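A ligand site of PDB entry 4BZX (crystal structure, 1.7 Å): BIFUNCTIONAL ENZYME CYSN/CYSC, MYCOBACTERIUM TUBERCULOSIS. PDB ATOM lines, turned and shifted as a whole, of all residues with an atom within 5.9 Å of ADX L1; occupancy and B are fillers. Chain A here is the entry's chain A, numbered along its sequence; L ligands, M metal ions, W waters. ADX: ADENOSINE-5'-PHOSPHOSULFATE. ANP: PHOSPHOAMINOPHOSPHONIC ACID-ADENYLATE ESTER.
Ser 13 touches ADX L1.
Gly 40 touches ADX L1.
Asp 41 touches ADX L1 (CB to O3', 3.5 Å).
Phe 53 touches ADX L1.
Leu 62 touches ADX L1 (CD2 to O1B, 3.5 Å).
CA of Ala 83 touches O2A of ADX L1, at 3.3 Å.
CD of Pro 86 touches O2B of ADX L1, at 3.3 Å.
Leu 125 touches ADX L1.
O of Thr 135 touches N6 of ADX L1 (3.7 Å).
CD1 of Phe 137 touches C6 of ADX L1 (3.3 Å).
OG1 of Thr 138 touches C2 of ADX L1, at 3.4 Å.
Hydrophobic or aromatic side chains within 4 Å of ADX L1: Phe 53, Leu 62, Ala 83, Ile 84, Pro 86, Leu 125 and Phe 137.
The nearest printed residue that does not touch ADX L1 is Ile 134 (4.3 Å).
The guanidinium group (NE) of Arg 44 is in salt-bridge range of an oxygen (O1A) of ADX L1 (2.8 Å).
O2B of ADX L1 is in salt-bridge range of NH1 of Arg 58 (2.8 Å).
An oxygen (O2A) of ADX L1 sits at hydrogen-bond distance from the backbone NH (N) of Ile 84 (2.9 Å).
The backbone carbonyl oxygen of His 136 is in hydrogen-bond range of a nitrogen (N6) of ADX L1, at 2.9 Å.
The side-chain amino group (NZ) of Lys 123 sits at hydrogen-bond distance from an oxygen (O3') of ADX L1, 2.9 Å away.
The side-chain amide nitrogen (ND2) of Asn 61 lies within hydrogen-bond range of an oxygen (O1A) of ADX L1 (3.0 Å).
The backbone NH (N) of Ser 85 sits at hydrogen-bond distance from an oxygen (O1B) of ADX L1, 3.0 Å away.
An oxygen (O1G) of ANP L2 lies within salt-bridge range of the side-chain amino group (NZ) of Lys 123 (3.5 Å).
OG of Ser 13 sits at hydrogen-bond distance from O1G of ANP L2, at 2.4 Å.
An oxygen (O1B) of ANP L2 lies within hydrogen-bond range of the backbone NH of Lys 17 (2.9 Å).
NZ of Lys 17 lies within salt-bridge range of O1B of ANP L2 (2.7 Å).
The guanidinium group (NH1) of Arg 44 is in hydrogen-bond range of the backbone carbonyl oxygen (O) of Gly 52.
The guanidinium group (NH2) of Arg 58 is in hydrogen-bond range of the backbone carbonyl oxygen (O) of His 136, at 3.0 Å.
The guanidinium group of Arg 58 sits at hydrogen-bond distance from the backbone carbonyl oxygen of Phe 53, at 2.9 Å.
NH1 of Arg 58 is in hydrogen-bond range of OG1 of Thr 138 (2.9 Å).
The side-chain hydroxyl of Ser 85 is in hydrogen-bond range of the backbone carbonyl oxygen of Ala 83 (3.4 Å).
OD1 of Asp 39 lies within hydrogen-bond range of N of Asp 41 (2.9 Å).
N of Gly 40 sits at hydrogen-bond distance from O of Pro 82.
An oxygen (O2') of ADX L1 is in hydrogen-bond range of an oxygen (O1G) of ANP L2 (2.7 Å).
Water W1 lies within hydrogen-bond range of the backbone carbonyl oxygen of Thr 135 (2.6 Å) and a nitrogen (N6) of ADX L1 (3.0 Å).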
ATOM      1  N   SER A  13       4.425  18.943  25.741  1.00  0.00           N
ATOM      2  CA  SER A  13       3.814  17.817  26.368  1.00  0.00           C
ATOM      3  C   SER A  13       2.536  18.224  27.096  1.00  0.00           C
ATOM      4  O   SER A  13       2.494  19.212  27.797  1.00  0.00           O
ATOM      5  CB  SER A  13       4.786  17.129  27.311  1.00  0.00           C
ATOM      6  OG  SER A  13       4.173  15.999  27.877  1.00  0.00           O
ATOM      7  N   LYS A  17      -1.920  17.044  21.496  1.00  0.00           N
ATOM      8  CA  LYS A  17      -1.576  16.562  20.142  1.00  0.00           C
ATOM      9  C   LYS A  17      -2.179  15.197  19.839  1.00  0.00           C
ATOM     10  O   LYS A  17      -2.820  15.006  18.796  1.00  0.00           O
ATOM     11  CB  LYS A  17      -0.057  16.496  19.964  1.00  0.00           C
ATOM     12  CG  LYS A  17       0.674  17.814  20.145  1.00  0.00           C
ATOM     13  CD  LYS A  17       2.199  17.708  19.997  1.00  0.00           C
ATOM     14  CE  LYS A  17       2.877  16.729  20.946  1.00  0.00           C
ATOM     15  NZ  LYS A  17       2.744  17.231  22.347  1.00  0.00           N
ATOM     16  N   ASP A  39       2.257   8.204  16.236  1.00  0.00           N
ATOM     17  CA  ASP A  39       2.400   8.962  17.504  1.00  0.00           C
ATOM     18  C   ASP A  39       3.806   8.821  18.032  1.00  0.00           C
ATOM     19  O   ASP A  39       4.285   7.682  18.226  1.00  0.00           O
ATOM     20  CB  ASP A  39       1.365   8.415  18.475  1.00  0.00           C
ATOM     21  CG  ASP A  39       1.306   9.172  19.825  1.00  0.00           C
ATOM     22  OD1 ASP A  39       2.273   9.125  20.595  1.00  0.00           O
ATOM     23  OD2 ASP A  39       0.260   9.747  20.115  1.00  0.00           O
ATOM     24  N   GLY A  40       4.492   9.913  18.243  1.00  0.00           N
ATOM     25  CA  GLY A  40       5.859   9.942  18.752  1.00  0.00           C
ATOM     26  C   GLY A  40       6.071   9.055  19.953  1.00  0.00           C
ATOM     27  O   GLY A  40       7.027   8.280  20.016  1.00  0.00           O
ATOM     28  N   ASP A  41       5.186   9.171  20.976  1.00  0.00           N
ATOM     29  CA  ASP A  41       5.320   8.313  22.136  1.00  0.00           C
ATOM     30  C   ASP A  41       5.197   6.827  21.794  1.00  0.00           C
ATOM     31  O   ASP A  41       5.943   5.970  22.332  1.00  0.00           O
ATOM     32  CB  ASP A  41       4.253   8.730  23.189  1.00  0.00           C
ATOM     33  CG  ASP A  41       4.400   7.985  24.500  1.00  0.00           C
ATOM     34  OD1 ASP A  41       5.419   8.101  25.167  1.00  0.00           O
ATOM     35  OD2 ASP A  41       3.482   7.277  24.880  1.00  0.00           O
ATOM     36  N   ARG A  44       8.182   5.462  19.949  1.00  0.00           N
ATOM     37  CA  ARG A  44       9.380   5.420  20.803  1.00  0.00           C
ATOM     38  C   ARG A  44       9.407   4.107  21.579  1.00  0.00           C
ATOM     39  O   ARG A  44      10.379   3.816  22.285  1.00  0.00           O
ATOM     40  CB  ARG A  44       9.505   6.613  21.762  1.00  0.00           C
ATOM     41  CG  ARG A  44      10.064   7.844  21.057  1.00  0.00           C
ATOM     42  CD  ARG A  44       9.937   9.067  21.938  1.00  0.00           C
ATOM     43  NE  ARG A  44      10.653  10.186  21.422  1.00  0.00           N
ATOM     44  CZ  ARG A  44      11.963  10.416  21.578  1.00  0.00           C
ATOM     45  NH1 ARG A  44      12.719   9.496  22.256  1.00  0.00           N
ATOM     46  NH2 ARG A  44      12.506  11.501  21.034  1.00  0.00           N
ATOM     47  N   GLY A  52      16.620   8.464  22.924  1.00  0.00           N
ATOM     48  CA  GLY A  52      16.210   9.239  24.082  1.00  0.00           C
ATOM     49  C   GLY A  52      15.782  10.663  23.713  1.00  0.00           C
ATOM     50  O   GLY A  52      15.163  10.903  22.668  1.00  0.00           O
ATOM     51  N   PHE A  53      16.087  11.578  24.638  1.00  0.00           N
ATOM     52  CA  PHE A  53      15.581  12.979  24.567  1.00  0.00           C
ATOM     53  C   PHE A  53      16.652  13.998  24.476  1.00  0.00           C
ATOM     54  O   PHE A  53      16.374  15.177  24.501  1.00  0.00           O
ATOM     55  CB  PHE A  53      14.613  13.211  25.728  1.00  0.00           C
ATOM     56  CG  PHE A  53      13.357  12.398  25.580  1.00  0.00           C
ATOM     57  CD1 PHE A  53      12.367  12.837  24.666  1.00  0.00           C
ATOM     58  CD2 PHE A  53      13.211  11.200  26.174  1.00  0.00           C
ATOM     59  CE1 PHE A  53      11.189  12.070  24.501  1.00  0.00           C
ATOM     60  CE2 PHE A  53      12.065  10.450  26.030  1.00  0.00           C
ATOM     61  CZ  PHE A  53      11.093  10.864  25.182  1.00  0.00           C
ATOM     62  N   ASP A  57      19.002  12.933  19.494  1.00  0.00           N
ATOM     63  CA  ASP A  57      18.048  11.826  19.438  1.00  0.00           C
ATOM     64  C   ASP A  57      16.648  12.282  19.012  1.00  0.00           C
ATOM     65  O   ASP A  57      15.991  11.590  18.235  1.00  0.00           O
ATOM     66  CB  ASP A  57      17.985  11.094  20.776  1.00  0.00           C
ATOM     67  CG  ASP A  57      19.129  10.130  20.956  1.00  0.00           C
ATOM     68  OD1 ASP A  57      20.029  10.056  20.065  1.00  0.00           O
ATOM     69  OD2 ASP A  57      19.122   9.390  21.961  1.00  0.00           O
ATOM     70  N   ARG A  58      16.222  13.466  19.484  1.00  0.00           N
ATOM     71  CA  ARG A  58      14.940  14.005  19.038  1.00  0.00           C
ATOM     72  C   ARG A  58      14.978  14.256  17.501  1.00  0.00           C
ATOM     73  O   ARG A  58      14.014  13.918  16.753  1.00  0.00           O
ATOM     74  CB  ARG A  58      14.541  15.244  19.793  1.00  0.00           C
ATOM     75  CG  ARG A  58      14.265  15.048  21.259  1.00  0.00           C
ATOM     76  CD  ARG A  58      14.030  16.393  21.871  1.00  0.00           C
ATOM     77  NE  ARG A  58      13.974  16.374  23.320  1.00  0.00           N
ATOM     78  CZ  ARG A  58      12.910  16.575  24.075  1.00  0.00           C
ATOM     79  NH1 ARG A  58      11.712  16.550  23.612  1.00  0.00           N
ATOM     80  NH2 ARG A  58      13.105  16.671  25.385  1.00  0.00           N
ATOM     81  N   ALA A  59      16.078  14.811  17.007  1.00  0.00           N
ATOM     82  CA  ALA A  59      16.193  15.072  15.565  1.00  0.00           C
ATOM     83  C   ALA A  59      16.085  13.812  14.736  1.00  0.00           C
ATOM     84  O   ALA A  59      15.413  13.821  13.692  1.00  0.00           O
ATOM     85  CB  ALA A  59      17.541  15.733  15.280  1.00  0.00           C
ATOM     86  N   ASN A  61      14.670  10.952  15.817  1.00  0.00           N
ATOM     87  CA  ASN A  61      13.307  10.453  15.995  1.00  0.00           C
ATOM     88  C   ASN A  61      12.380  11.051  14.933  1.00  0.00           C
ATOM     89  O   ASN A  61      11.666  10.328  14.260  1.00  0.00           O
ATOM     90  CB  ASN A  61      12.875  10.836  17.384  1.00  0.00           C
ATOM     91  CG  ASN A  61      11.465  10.431  17.705  1.00  0.00           C
ATOM     92  OD1 ASN A  61      11.121   9.231  17.677  1.00  0.00           O
ATOM     93  ND2 ASN A  61      10.640  11.441  18.004  1.00  0.00           N
ATOM     94  N   LEU A  62      12.485  12.351  14.781  1.00  0.00           N
ATOM     95  CA  LEU A  62      11.631  13.130  13.904  1.00  0.00           C
ATOM     96  C   LEU A  62      12.022  12.952  12.417  1.00  0.00           C
ATOM     97  O   LEU A  62      11.128  12.911  11.518  1.00  0.00           O
ATOM     98  CB  LEU A  62      11.613  14.528  14.359  1.00  0.00           C
ATOM     99  CG  LEU A  62      11.092  14.726  15.802  1.00  0.00           C
ATOM    100  CD1 LEU A  62      11.436  16.107  16.315  1.00  0.00           C
ATOM    101  CD2 LEU A  62       9.614  14.386  15.868  1.00  0.00           C
ATOM    102  N   LEU A  65      10.451   9.619  11.663  1.00  0.00           N
ATOM    103  CA  LEU A  65       9.014   9.786  11.546  1.00  0.00           C
ATOM    104  C   LEU A  65       8.626  10.486  10.233  1.00  0.00           C
ATOM    105  O   LEU A  65       7.619  10.153   9.635  1.00  0.00           O
ATOM    106  CB  LEU A  65       8.538  10.582  12.734  1.00  0.00           C
ATOM    107  CG  LEU A  65       8.469   9.881  14.072  1.00  0.00           C
ATOM    108  CD1 LEU A  65       7.922  10.850  15.123  1.00  0.00           C
ATOM    109  CD2 LEU A  65       7.597   8.620  13.895  1.00  0.00           C
ATOM    110  N   PRO A  82       1.466  13.254  15.831  1.00  0.00           N
ATOM    111  CA  PRO A  82       1.596  13.983  17.068  1.00  0.00           C
ATOM    112  C   PRO A  82       2.934  13.724  17.714  1.00  0.00           C
ATOM    113  O   PRO A  82       3.204  12.593  18.203  1.00  0.00           O
ATOM    114  CB  PRO A  82       0.443  13.465  17.876  1.00  0.00           C
ATOM    115  CG  PRO A  82       0.297  12.059  17.433  1.00  0.00           C
ATOM    116  CD  PRO A  82       0.511  12.111  15.993  1.00  0.00           C
ATOM    117  N   ALA A  83       3.816  14.699  17.609  1.00  0.00           N
ATOM    118  CA  ALA A  83       5.157  14.616  18.197  1.00  0.00           C
ATOM    119  C   ALA A  83       5.563  15.988  18.635  1.00  0.00           C
ATOM    120  O   ALA A  83       5.153  16.950  18.023  1.00  0.00           O
ATOM    121  CB  ALA A  83       6.142  14.133  17.220  1.00  0.00           C
ATOM    122  N   ILE A  84       6.240  16.119  19.770  1.00  0.00           N
ATOM    123  CA  ILE A  84       6.525  17.442  20.289  1.00  0.00           C
ATOM    124  C   ILE A  84       7.179  18.366  19.257  1.00  0.00           C
ATOM    125  O   ILE A  84       6.750  19.513  19.029  1.00  0.00           O
ATOM    126  CB  ILE A  84       7.363  17.330  21.612  1.00  0.00           C
ATOM    127  CG1 ILE A  84       6.484  16.805  22.738  1.00  0.00           C
ATOM    128  CG2 ILE A  84       7.951  18.719  22.002  1.00  0.00           C
ATOM    129  CD1 ILE A  84       7.320  16.498  23.969  1.00  0.00           C
ATOM    130  N   SER A  85       8.183  17.833  18.536  1.00  0.00           N
ATOM    131  CA  SER A  85       8.923  18.578  17.502  1.00  0.00           C
ATOM    132  C   SER A  85       9.410  19.949  18.007  1.00  0.00           C
ATOM    133  O   SER A  85       8.912  20.973  17.518  1.00  0.00           O
ATOM    134  CB  SER A  85       8.011  18.804  16.297  1.00  0.00           C
ATOM    135  OG  SER A  85       7.642  17.582  15.743  1.00  0.00           O
ATOM    136  N   PRO A  86      10.208  19.983  19.099  1.00  0.00           N
ATOM    137  CA  PRO A  86      10.453  21.227  19.824  1.00  0.00           C
ATOM    138  C   PRO A  86      11.219  22.350  19.071  1.00  0.00           C
ATOM    139  O   PRO A  86      11.041  23.529  19.394  1.00  0.00           O
ATOM    140  CB  PRO A  86      11.172  20.782  21.072  1.00  0.00           C
ATOM    141  CG  PRO A  86      11.882  19.468  20.679  1.00  0.00           C
ATOM    142  CD  PRO A  86      10.946  18.845  19.704  1.00  0.00           C
ATOM    143  N   HIS A  90      13.554  20.996  13.431  1.00  0.00           N
ATOM    144  CA  HIS A  90      12.829  19.719  13.377  1.00  0.00           C
ATOM    145  C   HIS A  90      11.630  19.783  12.450  1.00  0.00           C
ATOM    146  O   HIS A  90      11.456  18.910  11.586  1.00  0.00           O
ATOM    147  CB  HIS A  90      12.337  19.296  14.778  1.00  0.00           C
ATOM    148  CG  HIS A  90      13.415  19.066  15.767  1.00  0.00           C
ATOM    149  ND1 HIS A  90      13.231  19.117  17.126  1.00  0.00           N
ATOM    150  CD2 HIS A  90      14.725  18.781  15.578  1.00  0.00           C
ATOM    151  CE1 HIS A  90      14.366  18.841  17.728  1.00  0.00           C
ATOM    152  NE2 HIS A  90      15.284  18.618  16.799  1.00  0.00           N
ATOM    153  N   LYS A 123       0.482  12.461  32.596  1.00  0.00           N
ATOM    154  CA  LYS A 123       1.397  11.361  32.902  1.00  0.00           C
ATOM    155  C   LYS A 123       2.336  11.655  34.078  1.00  0.00           C
ATOM    156  O   LYS A 123       3.239  10.860  34.391  1.00  0.00           O
ATOM    157  CB  LYS A 123       2.238  11.077  31.654  1.00  0.00           C
ATOM    158  CG  LYS A 123       1.414  10.729  30.429  1.00  0.00           C
ATOM    159  CD  LYS A 123       2.283  10.616  29.166  1.00  0.00           C
ATOM    160  CE  LYS A 123       1.486  11.076  27.952  1.00  0.00           C
ATOM    161  NZ  LYS A 123       2.145  10.953  26.611  1.00  0.00           N
ATOM    162  N   LEU A 125       4.598  13.848  34.358  1.00  0.00           N
ATOM    163  CA  LEU A 125       5.952  14.190  33.927  1.00  0.00           C
ATOM    164  C   LEU A 125       6.364  15.589  34.321  1.00  0.00           C
ATOM    165  O   LEU A 125       7.525  15.800  34.644  1.00  0.00           O
ATOM    166  CB  LEU A 125       6.051  14.069  32.407  1.00  0.00           C
ATOM    167  CG  LEU A 125       5.942  12.615  31.910  1.00  0.00           C
ATOM    168  CD1 LEU A 125       6.046  12.573  30.392  1.00  0.00           C
ATOM    169  CD2 LEU A 125       6.967  11.746  32.532  1.00  0.00           C
ATOM    170  N   ILE A 134      13.289  13.789  36.400  1.00  0.00           N
ATOM    171  CA  ILE A 134      13.514  13.672  34.944  1.00  0.00           C
ATOM    172  C   ILE A 134      14.249  14.945  34.530  1.00  0.00           C
ATOM    173  O   ILE A 134      13.899  16.012  35.037  1.00  0.00           O
ATOM    174  CB  ILE A 134      12.181  13.653  34.160  1.00  0.00           C
ATOM    175  CG1 ILE A 134      11.329  12.443  34.555  1.00  0.00           C
ATOM    176  CG2 ILE A 134      12.390  13.569  32.654  1.00  0.00           C
ATOM    177  CD1 ILE A 134      10.001  12.419  33.829  1.00  0.00           C
ATOM    178  N   THR A 135      15.205  14.850  33.628  1.00  0.00           N
ATOM    179  CA  THR A 135      15.878  16.032  33.147  1.00  0.00           C
ATOM    180  C   THR A 135      15.655  16.191  31.626  1.00  0.00           C
ATOM    181  O   THR A 135      15.176  15.282  30.974  1.00  0.00           O
ATOM    182  CB  THR A 135      17.396  15.948  33.453  1.00  0.00           C
ATOM    183  OG1 THR A 135      17.927  14.834  32.810  1.00  0.00           O
ATOM    184  CG2 THR A 135      17.648  15.830  34.946  1.00  0.00           C
ATOM    185  N   HIS A 136      15.970  17.390  31.124  1.00  0.00           N
ATOM    186  CA  HIS A 136      15.860  17.677  29.686  1.00  0.00           C
ATOM    187  C   HIS A 136      14.411  17.479  29.229  1.00  0.00           C
ATOM    188  O   HIS A 136      14.145  16.941  28.178  1.00  0.00           O
ATOM    189  CB  HIS A 136      16.795  16.786  28.781  1.00  0.00           C
ATOM    190  CG  HIS A 136      18.249  16.846  29.152  1.00  0.00           C
ATOM    191  ND1 HIS A 136      19.013  17.974  28.988  1.00  0.00           N
ATOM    192  CD2 HIS A 136      19.057  15.944  29.765  1.00  0.00           C
ATOM    193  CE1 HIS A 136      20.237  17.775  29.450  1.00  0.00           C
ATOM    194  NE2 HIS A 136      20.286  16.547  29.945  1.00  0.00           N
ATOM    195  N   PHE A 137      13.495  17.934  30.056  1.00  0.00           N
ATOM    196  CA  PHE A 137      12.073  17.900  29.745  1.00  0.00           C
ATOM    197  C   PHE A 137      11.572  19.186  29.059  1.00  0.00           C
ATOM    198  O   PHE A 137      11.695  20.303  29.581  1.00  0.00           O
ATOM    199  CB  PHE A 137      11.245  17.654  31.034  1.00  0.00           C
ATOM    200  CG  PHE A 137       9.858  17.269  30.715  1.00  0.00           C
ATOM    201  CD1 PHE A 137       9.609  16.002  30.236  1.00  0.00           C
ATOM    202  CD2 PHE A 137       8.793  18.173  30.856  1.00  0.00           C
ATOM    203  CE1 PHE A 137       8.315  15.620  29.910  1.00  0.00           C
ATOM    204  CE2 PHE A 137       7.508  17.783  30.495  1.00  0.00           C
ATOM    205  CZ  PHE A 137       7.286  16.506  30.010  1.00  0.00           C
ATOM    206  N   THR A 138      11.003  19.000  27.872  1.00  0.00           N
ATOM    207  CA  THR A 138      10.537  20.134  27.070  1.00  0.00           C
ATOM    208  C   THR A 138       9.705  21.140  27.835  1.00  0.00           C
ATOM    209  O   THR A 138       8.764  20.752  28.484  1.00  0.00           O
ATOM    210  CB  THR A 138       9.733  19.603  25.886  1.00  0.00           C
ATOM    211  OG1 THR A 138      10.540  18.662  25.165  1.00  0.00           O
ATOM    212  CG2 THR A 138       9.295  20.740  25.003  1.00  0.00           C
HETATM  213  SB  ADX L   1      10.254  14.736  20.274  1.00  0.00           S
HETATM  214  O1B ADX L   1       9.364  15.193  19.244  1.00  0.00           O
HETATM  215  O2B ADX L   1      10.890  15.809  21.019  1.00  0.00           O
HETATM  216  O3B ADX L   1      11.261  13.745  19.810  1.00  0.00           O
HETATM  217  PA  ADX L   1       8.175  12.901  21.127  1.00  0.00           P
HETATM  218  O1A ADX L   1       8.732  11.832  20.233  1.00  0.00           O
HETATM  219  O2A ADX L   1       6.888  13.524  20.765  1.00  0.00           O
HETATM  220  O3A ADX L   1       9.371  13.993  21.344  1.00  0.00           O
HETATM  221  O5' ADX L   1       8.128  12.238  22.585  1.00  0.00           O
HETATM  222  C5' ADX L   1       7.504  12.992  23.588  1.00  0.00           C
HETATM  223  C4' ADX L   1       6.835  11.945  24.498  1.00  0.00           C
HETATM  224  O4' ADX L   1       7.764  11.460  25.484  1.00  0.00           O
HETATM  225  C3' ADX L   1       5.673  12.609  25.181  1.00  0.00           C
HETATM  226  O3' ADX L   1       4.574  11.675  25.112  1.00  0.00           O
HETATM  227  C2' ADX L   1       6.204  12.826  26.543  1.00  0.00           C
HETATM  228  O2' ADX L   1       5.079  12.641  27.423  1.00  0.00           O
HETATM  229  C1' ADX L   1       7.326  11.864  26.833  1.00  0.00           C
HETATM  230  N9  ADX L   1       8.599  12.316  27.372  1.00  0.00           N
HETATM  231  C8  ADX L   1       9.403  11.584  28.216  1.00  0.00           C
HETATM  232  N7  ADX L   1      10.528  12.217  28.497  1.00  0.00           N
HETATM  233  C5  ADX L   1      10.453  13.406  27.844  1.00  0.00           C
HETATM  234  C6  ADX L   1      11.334  14.549  27.805  1.00  0.00           C
HETATM  235  N6  ADX L   1      12.513  14.515  28.467  1.00  0.00           N
HETATM  236  N1  ADX L   1      10.925  15.592  27.042  1.00  0.00           N
HETATM  237  C2  ADX L   1       9.763  15.578  26.412  1.00  0.00           C
HETATM  238  N3  ADX L   1       8.869  14.548  26.428  1.00  0.00           N
HETATM  239  C4  ADX L   1       9.208  13.455  27.127  1.00  0.00           C
HETATM  240  PG  ANP L   2       2.608  14.374  25.052  1.00  0.00           P
HETATM  241  O1G ANP L   2       3.124  14.306  26.452  1.00  0.00           O
HETATM  242  O2G ANP L   2       2.287  12.991  24.538  1.00  0.00           O
HETATM  243  O3G ANP L   2       3.566  15.130  24.031  1.00  0.00           O
HETATM  244  PB  ANP L   2       0.015  15.455  24.010  1.00  0.00           P
HETATM  245  O1B ANP L   2       0.286  16.832  23.385  1.00  0.00           O
HETATM  246  O2B ANP L   2      -0.147  14.293  23.087  1.00  0.00           O
HETATM  247  N3B ANP L   2       1.081  15.107  25.186  1.00  0.00           N
HETATM  248  PA  ANP L   2      -2.548  14.588  25.070  1.00  0.00           P
HETATM  249  O1A ANP L   2      -2.036  13.324  25.700  1.00  0.00           O
HETATM  250  O2A ANP L   2      -3.297  14.454  23.787  1.00  0.00           O
HETATM  251  O3A ANP L   2      -1.356  15.639  24.949  1.00  0.00           O
HETATM  252  O5' ANP L   2      -3.480  15.506  26.070  1.00  0.00           O
HETATM  253  C5' ANP L   2      -3.160  15.923  27.358  1.00  0.00           C
HETATM  254  C4' ANP L   2      -4.520  16.205  28.030  1.00  0.00           C
HETATM  255  O4' ANP L   2      -4.973  17.449  27.673  1.00  0.00           O
HETATM  256  C3' ANP L   2      -5.570  15.209  27.576  1.00  0.00           C
HETATM  257  O3' ANP L   2      -5.746  14.265  28.640  1.00  0.00           O
HETATM  258  C2' ANP L   2      -6.800  16.009  27.319  1.00  0.00           C
HETATM  259  O2' ANP L   2      -7.803  15.585  28.220  1.00  0.00           O
HETATM  260  C1' ANP L   2      -6.412  17.412  27.601  1.00  0.00           C
HETATM  261  N9  ANP L   2      -6.929  18.208  26.503  1.00  0.00           N
HETATM  262  C8  ANP L   2      -6.316  18.373  25.289  1.00  0.00           C
HETATM  263  N7  ANP L   2      -7.049  19.194  24.493  1.00  0.00           N
HETATM  264  C5  ANP L   2      -8.155  19.537  25.202  1.00  0.00           C
HETATM  265  C6  ANP L   2      -9.346  20.384  24.984  1.00  0.00           C
HETATM  266  N6  ANP L   2      -9.495  21.000  23.800  1.00  0.00           N
HETATM  267  N1  ANP L   2     -10.260  20.504  25.997  1.00  0.00           N
HETATM  268  C2  ANP L   2     -10.116  19.864  27.180  1.00  0.00           C
HETATM  269  N3  ANP L   2      -9.051  19.097  27.454  1.00  0.00           N
HETATM  270  C4  ANP L   2      -8.071  18.898  26.526  1.00  0.00           C
HETATM  271 MG    MG M   1       0.936  12.536  23.026  1.00  0.00          MG
HETATM  272  O   HOH W   1      14.828  13.044  29.639  1.00  0.00           O
HETATM  273  O   HOH W   2      12.595  10.978  29.946  1.00  0.00           O
